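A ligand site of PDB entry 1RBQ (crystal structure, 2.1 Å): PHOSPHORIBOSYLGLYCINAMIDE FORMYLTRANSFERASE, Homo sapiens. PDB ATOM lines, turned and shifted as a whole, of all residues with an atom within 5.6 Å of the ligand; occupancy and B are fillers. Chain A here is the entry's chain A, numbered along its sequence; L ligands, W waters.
A nitrogen (N3) of the ligand sits at hydrogen-bond distance from the backbone carbonyl oxygen (O) of Glu 141 (3.0 Å).
A nitrogen (N4) of the ligand sits at hydrogen-bond distance from the backbone NH of Leu 92.
The backbone carbonyl oxygen (O) of Gly 117 lies within hydrogen-bond range of an oxygen (O6) of the ligand (3.1 Å).
The side-chain amide nitrogen of Asn 106 sits at hydrogen-bond distance from an oxygen (O5) of the ligand (3.1 Å).
ND1 of His 108 sits at hydrogen-bond distance from O5 of the ligand, 2.7 Å away.
N1 of the ligand is in hydrogen-bond range of O of Met 89 (2.9 Å).
The backbone carbonyl oxygen (O) of Arg 90 lies within hydrogen-bond range of a nitrogen (N5) of the ligand (2.8 Å).
The guanidinium group (NH2) of Arg 64 lies within salt-bridge range of an oxygen (O7) of the ligand.
O4 of the ligand sits at hydrogen-bond distance from N of Asp 144, 3.1 Å away.
A nitrogen (N2) of the ligand sits at hydrogen-bond distance from the backbone carbonyl oxygen of Ala 140, at 2.8 Å.
NH1 of Arg 90 is in salt-bridge range of O7 of the ligand (3.5 Å).
An oxygen (O5) of the ligand sits at hydrogen-bond distance from the side-chain carboxylate (OD1) of Asp 144 (2.5 Å).
N3 of the ligand sits at hydrogen-bond distance from O of Leu 92 (2.8 Å).
N of Ile 91 lies within hydrogen-bond range of O8 of the ligand, 2.8 Å away.
The guanidinium group (NH1) of Arg 64 is in hydrogen-bond range of the backbone carbonyl oxygen (O) of Ile 91, at 3.3 Å.
O of Leu 85 lies within hydrogen-bond range of N of Ile 107, 3.3 Å away.
The backbone NH (N) of Asn 106 is in hydrogen-bond range of the backbone carbonyl oxygen (O) of His 137 (3.0 Å).
The side-chain amide oxygen (OD1) of Asn 106 sits close to the backbone carbonyl oxygen (O) of Leu 85 (3.4 Å).
A ring nitrogen (ND1) of His 108 lies close to the side-chain carboxylate (OD2) of Asp 144 (3.2 Å).
OD2 of Asp 144 sits at hydrogen-bond distance from N of Gly 117.
Leu 85 touches the ligand.
Phe 88 touches the ligand.
Val 97 touches the ligand.
Pro 109 touches the ligand (CD to F3, 3.3 Å).
CA of Ser 118 touches F1 of the ligand, at 3.5 Å.
CE1 of His 137 touches O4 of the ligand, at 3.99 Å.
Val 139 touches the ligand (CG1 to C17, 3.7 Å).
Asp 142 touches the ligand (O to O4, 3.7 Å).
Val 143 touches the ligand.
Hydrophobic or aromatic side chains within 4 Å of the ligand: Leu 85, Met 89, Ile 91, Leu 92, Val 97, His 108, Pro 109, His 137, Val 139 and Val 143.
20 residues have an atom within 4 Å of the ligand: Arg 64, Leu 85, Phe 88, Met 89, Arg 90, Ile 91, Leu 92, Val 97, Asn 106, His 108, Pro 109, Gly 117, Ser 118, His 137, Val 139, Ala 140, Glu 141, Asp 142, Val 143 and Asp 144.
Along chain A the residues within 4 Å of the ligand span positions 64 to 144.
Water W7 lies within hydrogen-bond range of an oxygen (O2) of the ligand (2.5 Å) and the guanidinium group of Arg 90 (3.1 Å).
Water W6 lies within hydrogen-bond range of N5 of the ligand (2.6 Å), O of Phe 88 (2.7 Å) and O of Arg 90 (2.9 Å).
Water W10 lies within hydrogen-bond range of the side-chain hydroxyl of Ser 118 (2.7 Å) and an oxygen (O1) of the ligand (2.7 Å).
Water W8 bridges O of Ile 107 and N of Gly 87.
Water W4 lies within hydrogen-bond range of the side-chain amide oxygen of Asn 106 (2.7 Å), the backbone carbonyl oxygen of Phe 88 (2.8 Å) and the backbone NH of Gly 87 (3.5 Å).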
ATOM      1  N   LYS A  37     -34.808  -6.868 -15.708  1.00  0.00           N
ATOM      2  CA  LYS A  37     -34.234  -6.945 -17.064  1.00  0.00           C
ATOM      3  C   LYS A  37     -34.750  -8.188 -17.807  1.00  0.00           C
ATOM      4  O   LYS A  37     -34.864  -9.270 -17.233  1.00  0.00           O
ATOM      5  CB  LYS A  37     -32.695  -7.016 -17.006  1.00  0.00           C
ATOM      6  CG  LYS A  37     -31.976  -5.745 -16.582  1.00  0.00           C
ATOM      7  CD  LYS A  37     -30.798  -5.420 -17.529  1.00  0.00           C
ATOM      8  CE  LYS A  37     -29.450  -5.677 -16.869  1.00  0.00           C
ATOM      9  NZ  LYS A  37     -28.609  -4.412 -16.771  1.00  0.00           N
ATOM     10  N   ARG A  64     -38.139   5.780  -8.930  1.00  0.00           N
ATOM     11  CA  ARG A  64     -37.948   4.535  -8.193  1.00  0.00           C
ATOM     12  C   ARG A  64     -39.168   4.121  -7.393  1.00  0.00           C
ATOM     13  O   ARG A  64     -39.496   2.939  -7.321  1.00  0.00           O
ATOM     14  CB  ARG A  64     -36.717   4.611  -7.269  1.00  0.00           C
ATOM     15  CG  ARG A  64     -35.414   4.861  -7.996  1.00  0.00           C
ATOM     16  CD  ARG A  64     -34.176   4.746  -7.122  1.00  0.00           C
ATOM     17  NE  ARG A  64     -33.011   5.234  -7.855  1.00  0.00           N
ATOM     18  CZ  ARG A  64     -32.100   4.463  -8.426  1.00  0.00           C
ATOM     19  NH1 ARG A  64     -32.166   3.134  -8.344  1.00  0.00           N
ATOM     20  NH2 ARG A  64     -31.097   5.025  -9.092  1.00  0.00           N
ATOM     21  N   LEU A  85     -32.891 -10.610  -2.406  1.00  0.00           N
ATOM     22  CA  LEU A  85     -32.221  -9.901  -3.496  1.00  0.00           C
ATOM     23  C   LEU A  85     -30.996 -10.705  -3.885  1.00  0.00           C
ATOM     24  O   LEU A  85     -30.059 -10.839  -3.095  1.00  0.00           O
ATOM     25  CB  LEU A  85     -31.821  -8.453  -3.080  1.00  0.00           C
ATOM     26  CG  LEU A  85     -32.883  -7.519  -2.472  1.00  0.00           C
ATOM     27  CD1 LEU A  85     -32.429  -6.032  -2.482  1.00  0.00           C
ATOM     28  CD2 LEU A  85     -34.249  -7.642  -3.161  1.00  0.00           C
ATOM     29  N   GLY A  87     -28.409 -10.874  -6.792  1.00  0.00           N
ATOM     30  CA  GLY A  87     -27.878 -10.179  -7.964  1.00  0.00           C
ATOM     31  C   GLY A  87     -28.859  -9.154  -8.523  1.00  0.00           C
ATOM     32  O   GLY A  87     -28.794  -8.794  -9.702  1.00  0.00           O
ATOM     33  N   PHE A  88     -29.790  -8.684  -7.680  1.00  0.00           N
ATOM     34  CA  PHE A  88     -30.647  -7.572  -8.033  1.00  0.00           C
ATOM     35  C   PHE A  88     -29.861  -6.258  -8.013  1.00  0.00           C
ATOM     36  O   PHE A  88     -29.237  -5.924  -6.995  1.00  0.00           O
ATOM     37  CB  PHE A  88     -31.843  -7.504  -7.076  1.00  0.00           C
ATOM     38  CG  PHE A  88     -32.923  -6.539  -7.507  1.00  0.00           C
ATOM     39  CD1 PHE A  88     -33.605  -6.716  -8.704  1.00  0.00           C
ATOM     40  CD2 PHE A  88     -33.244  -5.431  -6.712  1.00  0.00           C
ATOM     41  CE1 PHE A  88     -34.604  -5.829  -9.113  1.00  0.00           C
ATOM     42  CE2 PHE A  88     -34.242  -4.534  -7.099  1.00  0.00           C
ATOM     43  CZ  PHE A  88     -34.922  -4.733  -8.299  1.00  0.00           C
ATOM     44  N   MET A  89     -29.912  -5.515  -9.106  1.00  0.00           N
ATOM     45  CA  MET A  89     -29.046  -4.327  -9.284  1.00  0.00           C
ATOM     46  C   MET A  89     -29.704  -2.951  -9.139  1.00  0.00           C
ATOM     47  O   MET A  89     -29.106  -1.932  -9.514  1.00  0.00           O
ATOM     48  CB  MET A  89     -28.318  -4.404 -10.618  1.00  0.00           C
ATOM     49  CG  MET A  89     -27.214  -5.442 -10.664  1.00  0.00           C
ATOM     50  SD  MET A  89     -25.957  -5.187  -9.387  1.00  0.00           S
ATOM     51  CE  MET A  89     -26.004  -6.801  -8.551  1.00  0.00           C
ATOM     52  N   ARG A  90     -30.930  -2.906  -8.612  1.00  0.00           N
ATOM     53  CA  ARG A  90     -31.631  -1.628  -8.458  1.00  0.00           C
ATOM     54  C   ARG A  90     -31.707  -1.240  -6.993  1.00  0.00           C
ATOM     55  O   ARG A  90     -32.171  -2.021  -6.169  1.00  0.00           O
ATOM     56  CB  ARG A  90     -33.047  -1.676  -9.062  1.00  0.00           C
ATOM     57  CG  ARG A  90     -33.134  -1.845 -10.573  1.00  0.00           C
ATOM     58  CD  ARG A  90     -32.274  -0.883 -11.370  1.00  0.00           C
ATOM     59  NE  ARG A  90     -32.712   0.496 -11.230  1.00  0.00           N
ATOM     60  CZ  ARG A  90     -32.049   1.545 -11.705  1.00  0.00           C
ATOM     61  NH1 ARG A  90     -30.909   1.356 -12.375  1.00  0.00           N
ATOM     62  NH2 ARG A  90     -32.528   2.772 -11.532  1.00  0.00           N
ATOM     63  N   ILE A  91     -31.275  -0.027  -6.681  1.00  0.00           N
ATOM     64  CA  ILE A  91     -31.438   0.484  -5.325  1.00  0.00           C
ATOM     65  C   ILE A  91     -32.912   0.778  -5.072  1.00  0.00           C
ATOM     66  O   ILE A  91     -33.565   1.417  -5.880  1.00  0.00           O
ATOM     67  CB  ILE A  91     -30.528   1.709  -5.082  1.00  0.00           C
ATOM     68  CG1 ILE A  91     -29.057   1.276  -5.139  1.00  0.00           C
ATOM     69  CG2 ILE A  91     -30.853   2.388  -3.719  1.00  0.00           C
ATOM     70  CD1 ILE A  91     -28.103   2.441  -5.368  1.00  0.00           C
ATOM     71  N   LEU A  92     -33.433   0.260  -3.965  1.00  0.00           N
ATOM     72  CA  LEU A  92     -34.866   0.404  -3.644  1.00  0.00           C
ATOM     73  C   LEU A  92     -35.144   1.666  -2.811  1.00  0.00           C
ATOM     74  O   LEU A  92     -34.316   2.058  -1.990  1.00  0.00           O
ATOM     75  CB  LEU A  92     -35.371  -0.854  -2.940  1.00  0.00           C
ATOM     76  CG  LEU A  92     -35.398  -2.164  -3.746  1.00  0.00           C
ATOM     77  CD1 LEU A  92     -35.371  -3.399  -2.833  1.00  0.00           C
ATOM     78  CD2 LEU A  92     -36.614  -2.213  -4.682  1.00  0.00           C
ATOM     79  N   SER A  93     -36.298   2.285  -3.044  1.00  0.00           N
ATOM     80  CA  SER A  93     -36.667   3.525  -2.349  1.00  0.00           C
ATOM     81  C   SER A  93     -36.974   3.283  -0.880  1.00  0.00           C
ATOM     82  O   SER A  93     -37.271   2.157  -0.459  1.00  0.00           O
ATOM     83  CB  SER A  93     -37.873   4.206  -3.017  1.00  0.00           C
ATOM     84  OG  SER A  93     -39.044   3.391  -2.922  1.00  0.00           O
ATOM     85  N   VAL A  97     -38.362  -0.221   1.254  1.00  0.00           N
ATOM     86  CA  VAL A  97     -37.433  -0.803   2.223  1.00  0.00           C
ATOM     87  C   VAL A  97     -38.047  -0.840   3.631  1.00  0.00           C
ATOM     88  O   VAL A  97     -37.985  -1.868   4.322  1.00  0.00           O
ATOM     89  CB  VAL A  97     -36.047  -0.067   2.217  1.00  0.00           C
ATOM     90  CG1 VAL A  97     -35.193  -0.456   3.416  1.00  0.00           C
ATOM     91  CG2 VAL A  97     -35.308  -0.346   0.922  1.00  0.00           C
ATOM     92  N   ASN A 106     -30.337  -9.546   1.307  1.00  0.00           N
ATOM     93  CA  ASN A 106     -29.478  -9.347   0.151  1.00  0.00           C
ATOM     94  C   ASN A 106     -28.199 -10.142   0.313  1.00  0.00           C
ATOM     95  O   ASN A 106     -27.745 -10.375   1.440  1.00  0.00           O
ATOM     96  CB  ASN A 106     -29.121  -7.863  -0.010  1.00  0.00           C
ATOM     97  CG  ASN A 106     -28.225  -7.599  -1.206  1.00  0.00           C
ATOM     98  OD1 ASN A 106     -28.598  -7.896  -2.352  1.00  0.00           O
ATOM     99  ND2 ASN A 106     -27.031  -7.070  -0.958  1.00  0.00           N
ATOM    100  N   ILE A 107     -27.631 -10.581  -0.803  1.00  0.00           N
ATOM    101  CA  ILE A 107     -26.336 -11.248  -0.813  1.00  0.00           C
ATOM    102  C   ILE A 107     -25.333 -10.258  -1.364  1.00  0.00           C
ATOM    103  O   ILE A 107     -25.550  -9.687  -2.437  1.00  0.00           O
ATOM    104  CB  ILE A 107     -26.365 -12.591  -1.663  1.00  0.00           C
ATOM    105  CG1 ILE A 107     -24.999 -13.289  -1.684  1.00  0.00           C
ATOM    106  CG2 ILE A 107     -26.815 -12.353  -3.100  1.00  0.00           C
ATOM    107  CD1 ILE A 107     -24.486 -13.688  -0.277  1.00  0.00           C
ATOM    108  N   HIS A 108     -24.251 -10.017  -0.637  1.00  0.00           N
ATOM    109  CA  HIS A 108     -23.249  -9.046  -1.108  1.00  0.00           C
ATOM    110  C   HIS A 108     -21.849  -9.674  -1.139  1.00  0.00           C
ATOM    111  O   HIS A 108     -21.449 -10.249  -0.132  1.00  0.00           O
ATOM    112  CB  HIS A 108     -23.254  -7.772  -0.249  1.00  0.00           C
ATOM    113  CG  HIS A 108     -22.175  -6.805  -0.623  1.00  0.00           C
ATOM    114  ND1 HIS A 108     -22.321  -5.903  -1.661  1.00  0.00           N
ATOM    115  CD2 HIS A 108     -20.915  -6.651  -0.172  1.00  0.00           C
ATOM    116  CE1 HIS A 108     -21.202  -5.214  -1.802  1.00  0.00           C
ATOM    117  NE2 HIS A 108     -20.330  -5.656  -0.915  1.00  0.00           N
ATOM    118  N   PRO A 109     -21.130  -9.597  -2.264  1.00  0.00           N
ATOM    119  CA  PRO A 109     -19.827 -10.278  -2.393  1.00  0.00           C
ATOM    120  C   PRO A 109     -18.584  -9.573  -1.796  1.00  0.00           C
ATOM    121  O   PRO A 109     -17.558  -9.475  -2.477  1.00  0.00           O
ATOM    122  CB  PRO A 109     -19.676 -10.454  -3.923  1.00  0.00           C
ATOM    123  CG  PRO A 109     -20.374  -9.258  -4.497  1.00  0.00           C
ATOM    124  CD  PRO A 109     -21.544  -8.977  -3.540  1.00  0.00           C
ATOM    125  N   LYS A 116     -18.337  -1.804   0.061  1.00  0.00           N
ATOM    126  CA  LYS A 116     -19.740  -1.569  -0.270  1.00  0.00           C
ATOM    127  C   LYS A 116     -19.822  -1.230  -1.760  1.00  0.00           C
ATOM    128  O   LYS A 116     -18.869  -0.712  -2.333  1.00  0.00           O
ATOM    129  CB  LYS A 116     -20.286  -0.392   0.534  1.00  0.00           C
ATOM    130  CG  LYS A 116     -20.393  -0.656   2.024  1.00  0.00           C
ATOM    131  CD  LYS A 116     -20.890   0.612   2.759  1.00  0.00           C
ATOM    132  CE  LYS A 116     -21.015   0.347   4.241  1.00  0.00           C
ATOM    133  NZ  LYS A 116     -21.722   1.465   4.943  1.00  0.00           N
ATOM    134  N   GLY A 117     -20.957  -1.549  -2.383  1.00  0.00           N
ATOM    135  CA  GLY A 117     -21.128  -1.263  -3.789  1.00  0.00           C
ATOM    136  C   GLY A 117     -21.081  -2.486  -4.698  1.00  0.00           C
ATOM    137  O   GLY A 117     -20.630  -3.585  -4.293  1.00  0.00           O
ATOM    138  N   SER A 118     -21.509  -2.281  -5.933  1.00  0.00           N
ATOM    139  CA  SER A 118     -21.701  -3.351  -6.906  1.00  0.00           C
ATOM    140  C   SER A 118     -20.395  -3.904  -7.502  1.00  0.00           C
ATOM    141  O   SER A 118     -20.413  -4.967  -8.150  1.00  0.00           O
ATOM    142  CB  SER A 118     -22.585  -2.862  -8.046  1.00  0.00           C
ATOM    143  OG  SER A 118     -21.921  -1.838  -8.774  1.00  0.00           O
ATOM    144  N   HIS A 137     -27.186  -9.844   4.466  1.00  0.00           N
ATOM    145  CA  HIS A 137     -27.660  -8.831   5.394  1.00  0.00           C
ATOM    146  C   HIS A 137     -29.118  -8.467   5.177  1.00  0.00           C
ATOM    147  O   HIS A 137     -29.622  -8.580   4.066  1.00  0.00           O
ATOM    148  CB  HIS A 137     -26.757  -7.580   5.325  1.00  0.00           C
ATOM    149  CG  HIS A 137     -26.785  -6.896   3.986  1.00  0.00           C
ATOM    150  ND1 HIS A 137     -27.614  -5.823   3.721  1.00  0.00           N
ATOM    151  CD2 HIS A 137     -26.102  -7.149   2.842  1.00  0.00           C
ATOM    152  CE1 HIS A 137     -27.429  -5.432   2.467  1.00  0.00           C
ATOM    153  NE2 HIS A 137     -26.515  -6.214   1.914  1.00  0.00           N
ATOM    154  N   VAL A 139     -31.877  -5.734   4.450  1.00  0.00           N
ATOM    155  CA  VAL A 139     -31.733  -4.582   3.577  1.00  0.00           C
ATOM    156  C   VAL A 139     -32.196  -3.352   4.363  1.00  0.00           C
ATOM    157  O   VAL A 139     -33.323  -3.323   4.890  1.00  0.00           O
ATOM    158  CB  VAL A 139     -32.524  -4.754   2.229  1.00  0.00           C
ATOM    159  CG1 VAL A 139     -32.619  -3.453   1.441  1.00  0.00           C
ATOM    160  CG2 VAL A 139     -31.903  -5.854   1.371  1.00  0.00           C
ATOM    161  N   ALA A 140     -31.316  -2.358   4.467  1.00  0.00           N
ATOM    162  CA  ALA A 140     -31.700  -1.072   5.016  1.00  0.00           C
ATOM    163  C   ALA A 140     -31.687  -0.040   3.906  1.00  0.00           C
ATOM    164  O   ALA A 140     -31.248  -0.326   2.799  1.00  0.00           O
ATOM    165  CB  ALA A 140     -30.757  -0.662   6.174  1.00  0.00           C
ATOM    166  N   GLU A 141     -32.176   1.160   4.203  1.00  0.00           N
ATOM    167  CA  GLU A 141     -32.192   2.252   3.228  1.00  0.00           C
ATOM    168  C   GLU A 141     -30.803   2.518   2.701  1.00  0.00           C
ATOM    169  O   GLU A 141     -30.595   2.644   1.492  1.00  0.00           O
ATOM    170  CB  GLU A 141     -32.756   3.520   3.841  1.00  0.00           C
ATOM    171  CG  GLU A 141     -34.138   3.857   3.303  1.00  0.00           C
ATOM    172  CD  GLU A 141     -34.526   5.291   3.551  1.00  0.00           C
ATOM    173  OE1 GLU A 141     -35.185   5.552   4.588  1.00  0.00           O
ATOM    174  OE2 GLU A 141     -34.188   6.172   2.706  1.00  0.00           O
ATOM    175  N   ASP A 142     -29.849   2.584   3.612  1.00  0.00           N
ATOM    176  CA  ASP A 142     -28.461   2.763   3.244  1.00  0.00           C
ATOM    177  C   ASP A 142     -27.944   1.515   2.561  1.00  0.00           C
ATOM    178  O   ASP A 142     -28.048   0.406   3.089  1.00  0.00           O
ATOM    179  CB  ASP A 142     -27.620   3.118   4.465  1.00  0.00           C
ATOM    180  CG  ASP A 142     -27.129   4.536   4.426  1.00  0.00           C
ATOM    181  OD1 ASP A 142     -27.955   5.461   4.641  1.00  0.00           O
ATOM    182  OD2 ASP A 142     -25.941   4.816   4.159  1.00  0.00           O
ATOM    183  N   VAL A 143     -27.390   1.716   1.378  1.00  0.00           N
ATOM    184  CA  VAL A 143     -26.925   0.634   0.526  1.00  0.00           C
ATOM    185  C   VAL A 143     -25.863  -0.207   1.261  1.00  0.00           C
ATOM    186  O   VAL A 143     -24.963   0.347   1.906  1.00  0.00           O
ATOM    187  CB  VAL A 143     -26.382   1.194  -0.810  1.00  0.00           C
ATOM    188  CG1 VAL A 143     -25.693   0.099  -1.623  1.00  0.00           C
ATOM    189  CG2 VAL A 143     -27.525   1.853  -1.595  1.00  0.00           C
ATOM    190  N   ASP A 144     -26.023  -1.532   1.185  1.00  0.00           N
ATOM    191  CA  ASP A 144     -25.025  -2.474   1.725  1.00  0.00           C
ATOM    192  C   ASP A 144     -24.650  -2.183   3.168  1.00  0.00           C
ATOM    193  O   ASP A 144     -23.507  -2.362   3.565  1.00  0.00           O
ATOM    194  CB  ASP A 144     -23.761  -2.469   0.858  1.00  0.00           C
ATOM    195  CG  ASP A 144     -23.975  -3.145  -0.448  1.00  0.00           C
ATOM    196  OD1 ASP A 144     -24.885  -4.006  -0.519  1.00  0.00           O
ATOM    197  OD2 ASP A 144     -23.279  -2.876  -1.461  1.00  0.00           O
ATOM    198  N   ALA A 145     -25.637  -1.707   3.939  1.00  0.00           N
ATOM    199  CA  ALA A 145     -25.373  -1.268   5.298  1.00  0.00           C
ATOM    200  C   ALA A 145     -26.400  -1.780   6.313  1.00  0.00           C
ATOM    201  O   ALA A 145     -26.389  -1.362   7.455  1.00  0.00           O
ATOM    202  CB  ALA A 145     -25.252   0.268   5.346  1.00  0.00           C
ATOM    203  N   GLY A 146     -27.257  -2.712   5.901  1.00  0.00           N
ATOM    204  CA  GLY A 146     -28.206  -3.323   6.823  1.00  0.00           C
ATOM    205  C   GLY A 146     -27.534  -4.317   7.763  1.00  0.00           C
ATOM    206  O   GLY A 146     -26.344  -4.628   7.614  1.00  0.00           O
HETATM  207  O1  LIG L   1     -24.769  -0.938 -12.672  1.00  0.00           O
HETATM  208  C1  LIG L   1     -25.991  -0.463 -12.588  1.00  0.00           C
HETATM  209  O2  LIG L   1     -26.886  -0.571 -13.429  1.00  0.00           O
HETATM  210  C2  LIG L   1     -26.133   0.257 -11.321  1.00  0.00           C
HETATM  211  C3  LIG L   1     -27.558   0.712 -11.021  1.00  0.00           C
HETATM  212  C4  LIG L   1     -27.685   1.395  -9.711  1.00  0.00           C
HETATM  213  N1  LIG L   1     -27.420   0.327  -8.683  1.00  0.00           N
HETATM  214  C5  LIG L   1     -26.384   0.441  -7.765  1.00  0.00           C
HETATM  215  O3  LIG L   1     -25.595   1.381  -7.773  1.00  0.00           O
HETATM  216  C6  LIG L   1     -26.224  -0.653  -6.843  1.00  0.00           C
HETATM  217  C7  LIG L   1     -25.377  -0.405  -5.629  1.00  0.00           C
HETATM  218  C8  LIG L   1     -25.270  -1.416  -4.617  1.00  0.00           C
HETATM  219  C9  LIG L   1     -26.044  -2.715  -4.867  1.00  0.00           C
HETATM  220  C10 LIG L   1     -26.851  -2.927  -6.076  1.00  0.00           C
HETATM  221  C11 LIG L   1     -26.957  -1.934  -7.062  1.00  0.00           C
HETATM  222  C12 LIG L   1     -26.087  -4.132  -4.055  1.00  0.00           C
HETATM  223  C13 LIG L   1     -27.319  -4.483  -3.206  1.00  0.00           C
HETATM  224  C14 LIG L   1     -28.123  -3.150  -2.622  1.00  0.00           C
HETATM  225  C15 LIG L   1     -29.162  -3.794  -1.643  1.00  0.00           C
HETATM  226  C16 LIG L   1     -30.098  -2.661  -1.542  1.00  0.00           C
HETATM  227  C17 LIG L   1     -29.822  -1.971  -0.405  1.00  0.00           C
HETATM  228  O4  LIG L   1     -28.989  -2.223   0.681  1.00  0.00           O
HETATM  229  N2  LIG L   1     -30.553  -0.636   0.086  1.00  0.00           N
HETATM  230  C18 LIG L   1     -31.536  -0.179  -0.750  1.00  0.00           C
HETATM  231  N3  LIG L   1     -32.123   1.014  -0.527  1.00  0.00           N
HETATM  232  N4  LIG L   1     -31.838  -0.850  -1.855  1.00  0.00           N
HETATM  233  C19 LIG L   1     -31.190  -2.058  -2.314  1.00  0.00           C
HETATM  234  N5  LIG L   1     -31.610  -2.692  -3.475  1.00  0.00           N
HETATM  235  C20 LIG L   1     -24.924  -5.094  -3.641  1.00  0.00           C
HETATM  236  O5  LIG L   1     -24.839  -5.545  -2.548  1.00  0.00           O
HETATM  237  O6  LIG L   1     -23.670  -4.137  -3.788  1.00  0.00           O
HETATM  238  C21 LIG L   1     -24.631  -5.901  -4.893  1.00  0.00           C
HETATM  239  F1  LIG L   1     -24.515  -5.240  -6.112  1.00  0.00           F
HETATM  240  F2  LIG L   1     -25.828  -6.453  -4.984  1.00  0.00           F
HETATM  241  F3  LIG L   1     -23.634  -6.749  -4.684  1.00  0.00           F
HETATM  242  C22 LIG L   1     -29.091   2.073  -9.447  1.00  0.00           C
HETATM  243  O7  LIG L   1     -29.238   3.206  -9.878  1.00  0.00           O
HETATM  244  O8  LIG L   1     -30.096   1.431  -8.795  1.00  0.00           O
HETATM  245  O   HOH W   1     -23.081   1.786  -4.263  1.00  0.00           O
HETATM  246  O   HOH W   2     -23.459  -0.620 -14.821  1.00  0.00           O
HETATM  247  O   HOH W   3     -21.910  -7.652  -7.207  1.00  0.00           O
HETATM  248  O   HOH W   4     -28.827  -7.909  -5.052  1.00  0.00           O
HETATM  249  O   HOH W   5     -22.993   1.500  -8.563  1.00  0.00           O
HETATM  250  O   HOH W   6     -30.258  -4.018  -5.313  1.00  0.00           O
HETATM  251  O   HOH W   7     -29.339  -0.961 -13.606  1.00  0.00           O
HETATM  252  O   HOH W   8     -26.673  -9.415  -4.861  1.00  0.00           O
HETATM  253  O   HOH W   9     -24.405  -9.698  -6.306  1.00  0.00           O
HETATM  254  O   HOH W  10     -22.960  -0.409 -10.758  1.00  0.00           O
HETATM  255  O   HOH W  11     -28.684  -2.141   3.374  1.00  0.00           O
HETATM  256  O   HOH W  12     -25.645   4.006  -7.119  1.00  0.00           O
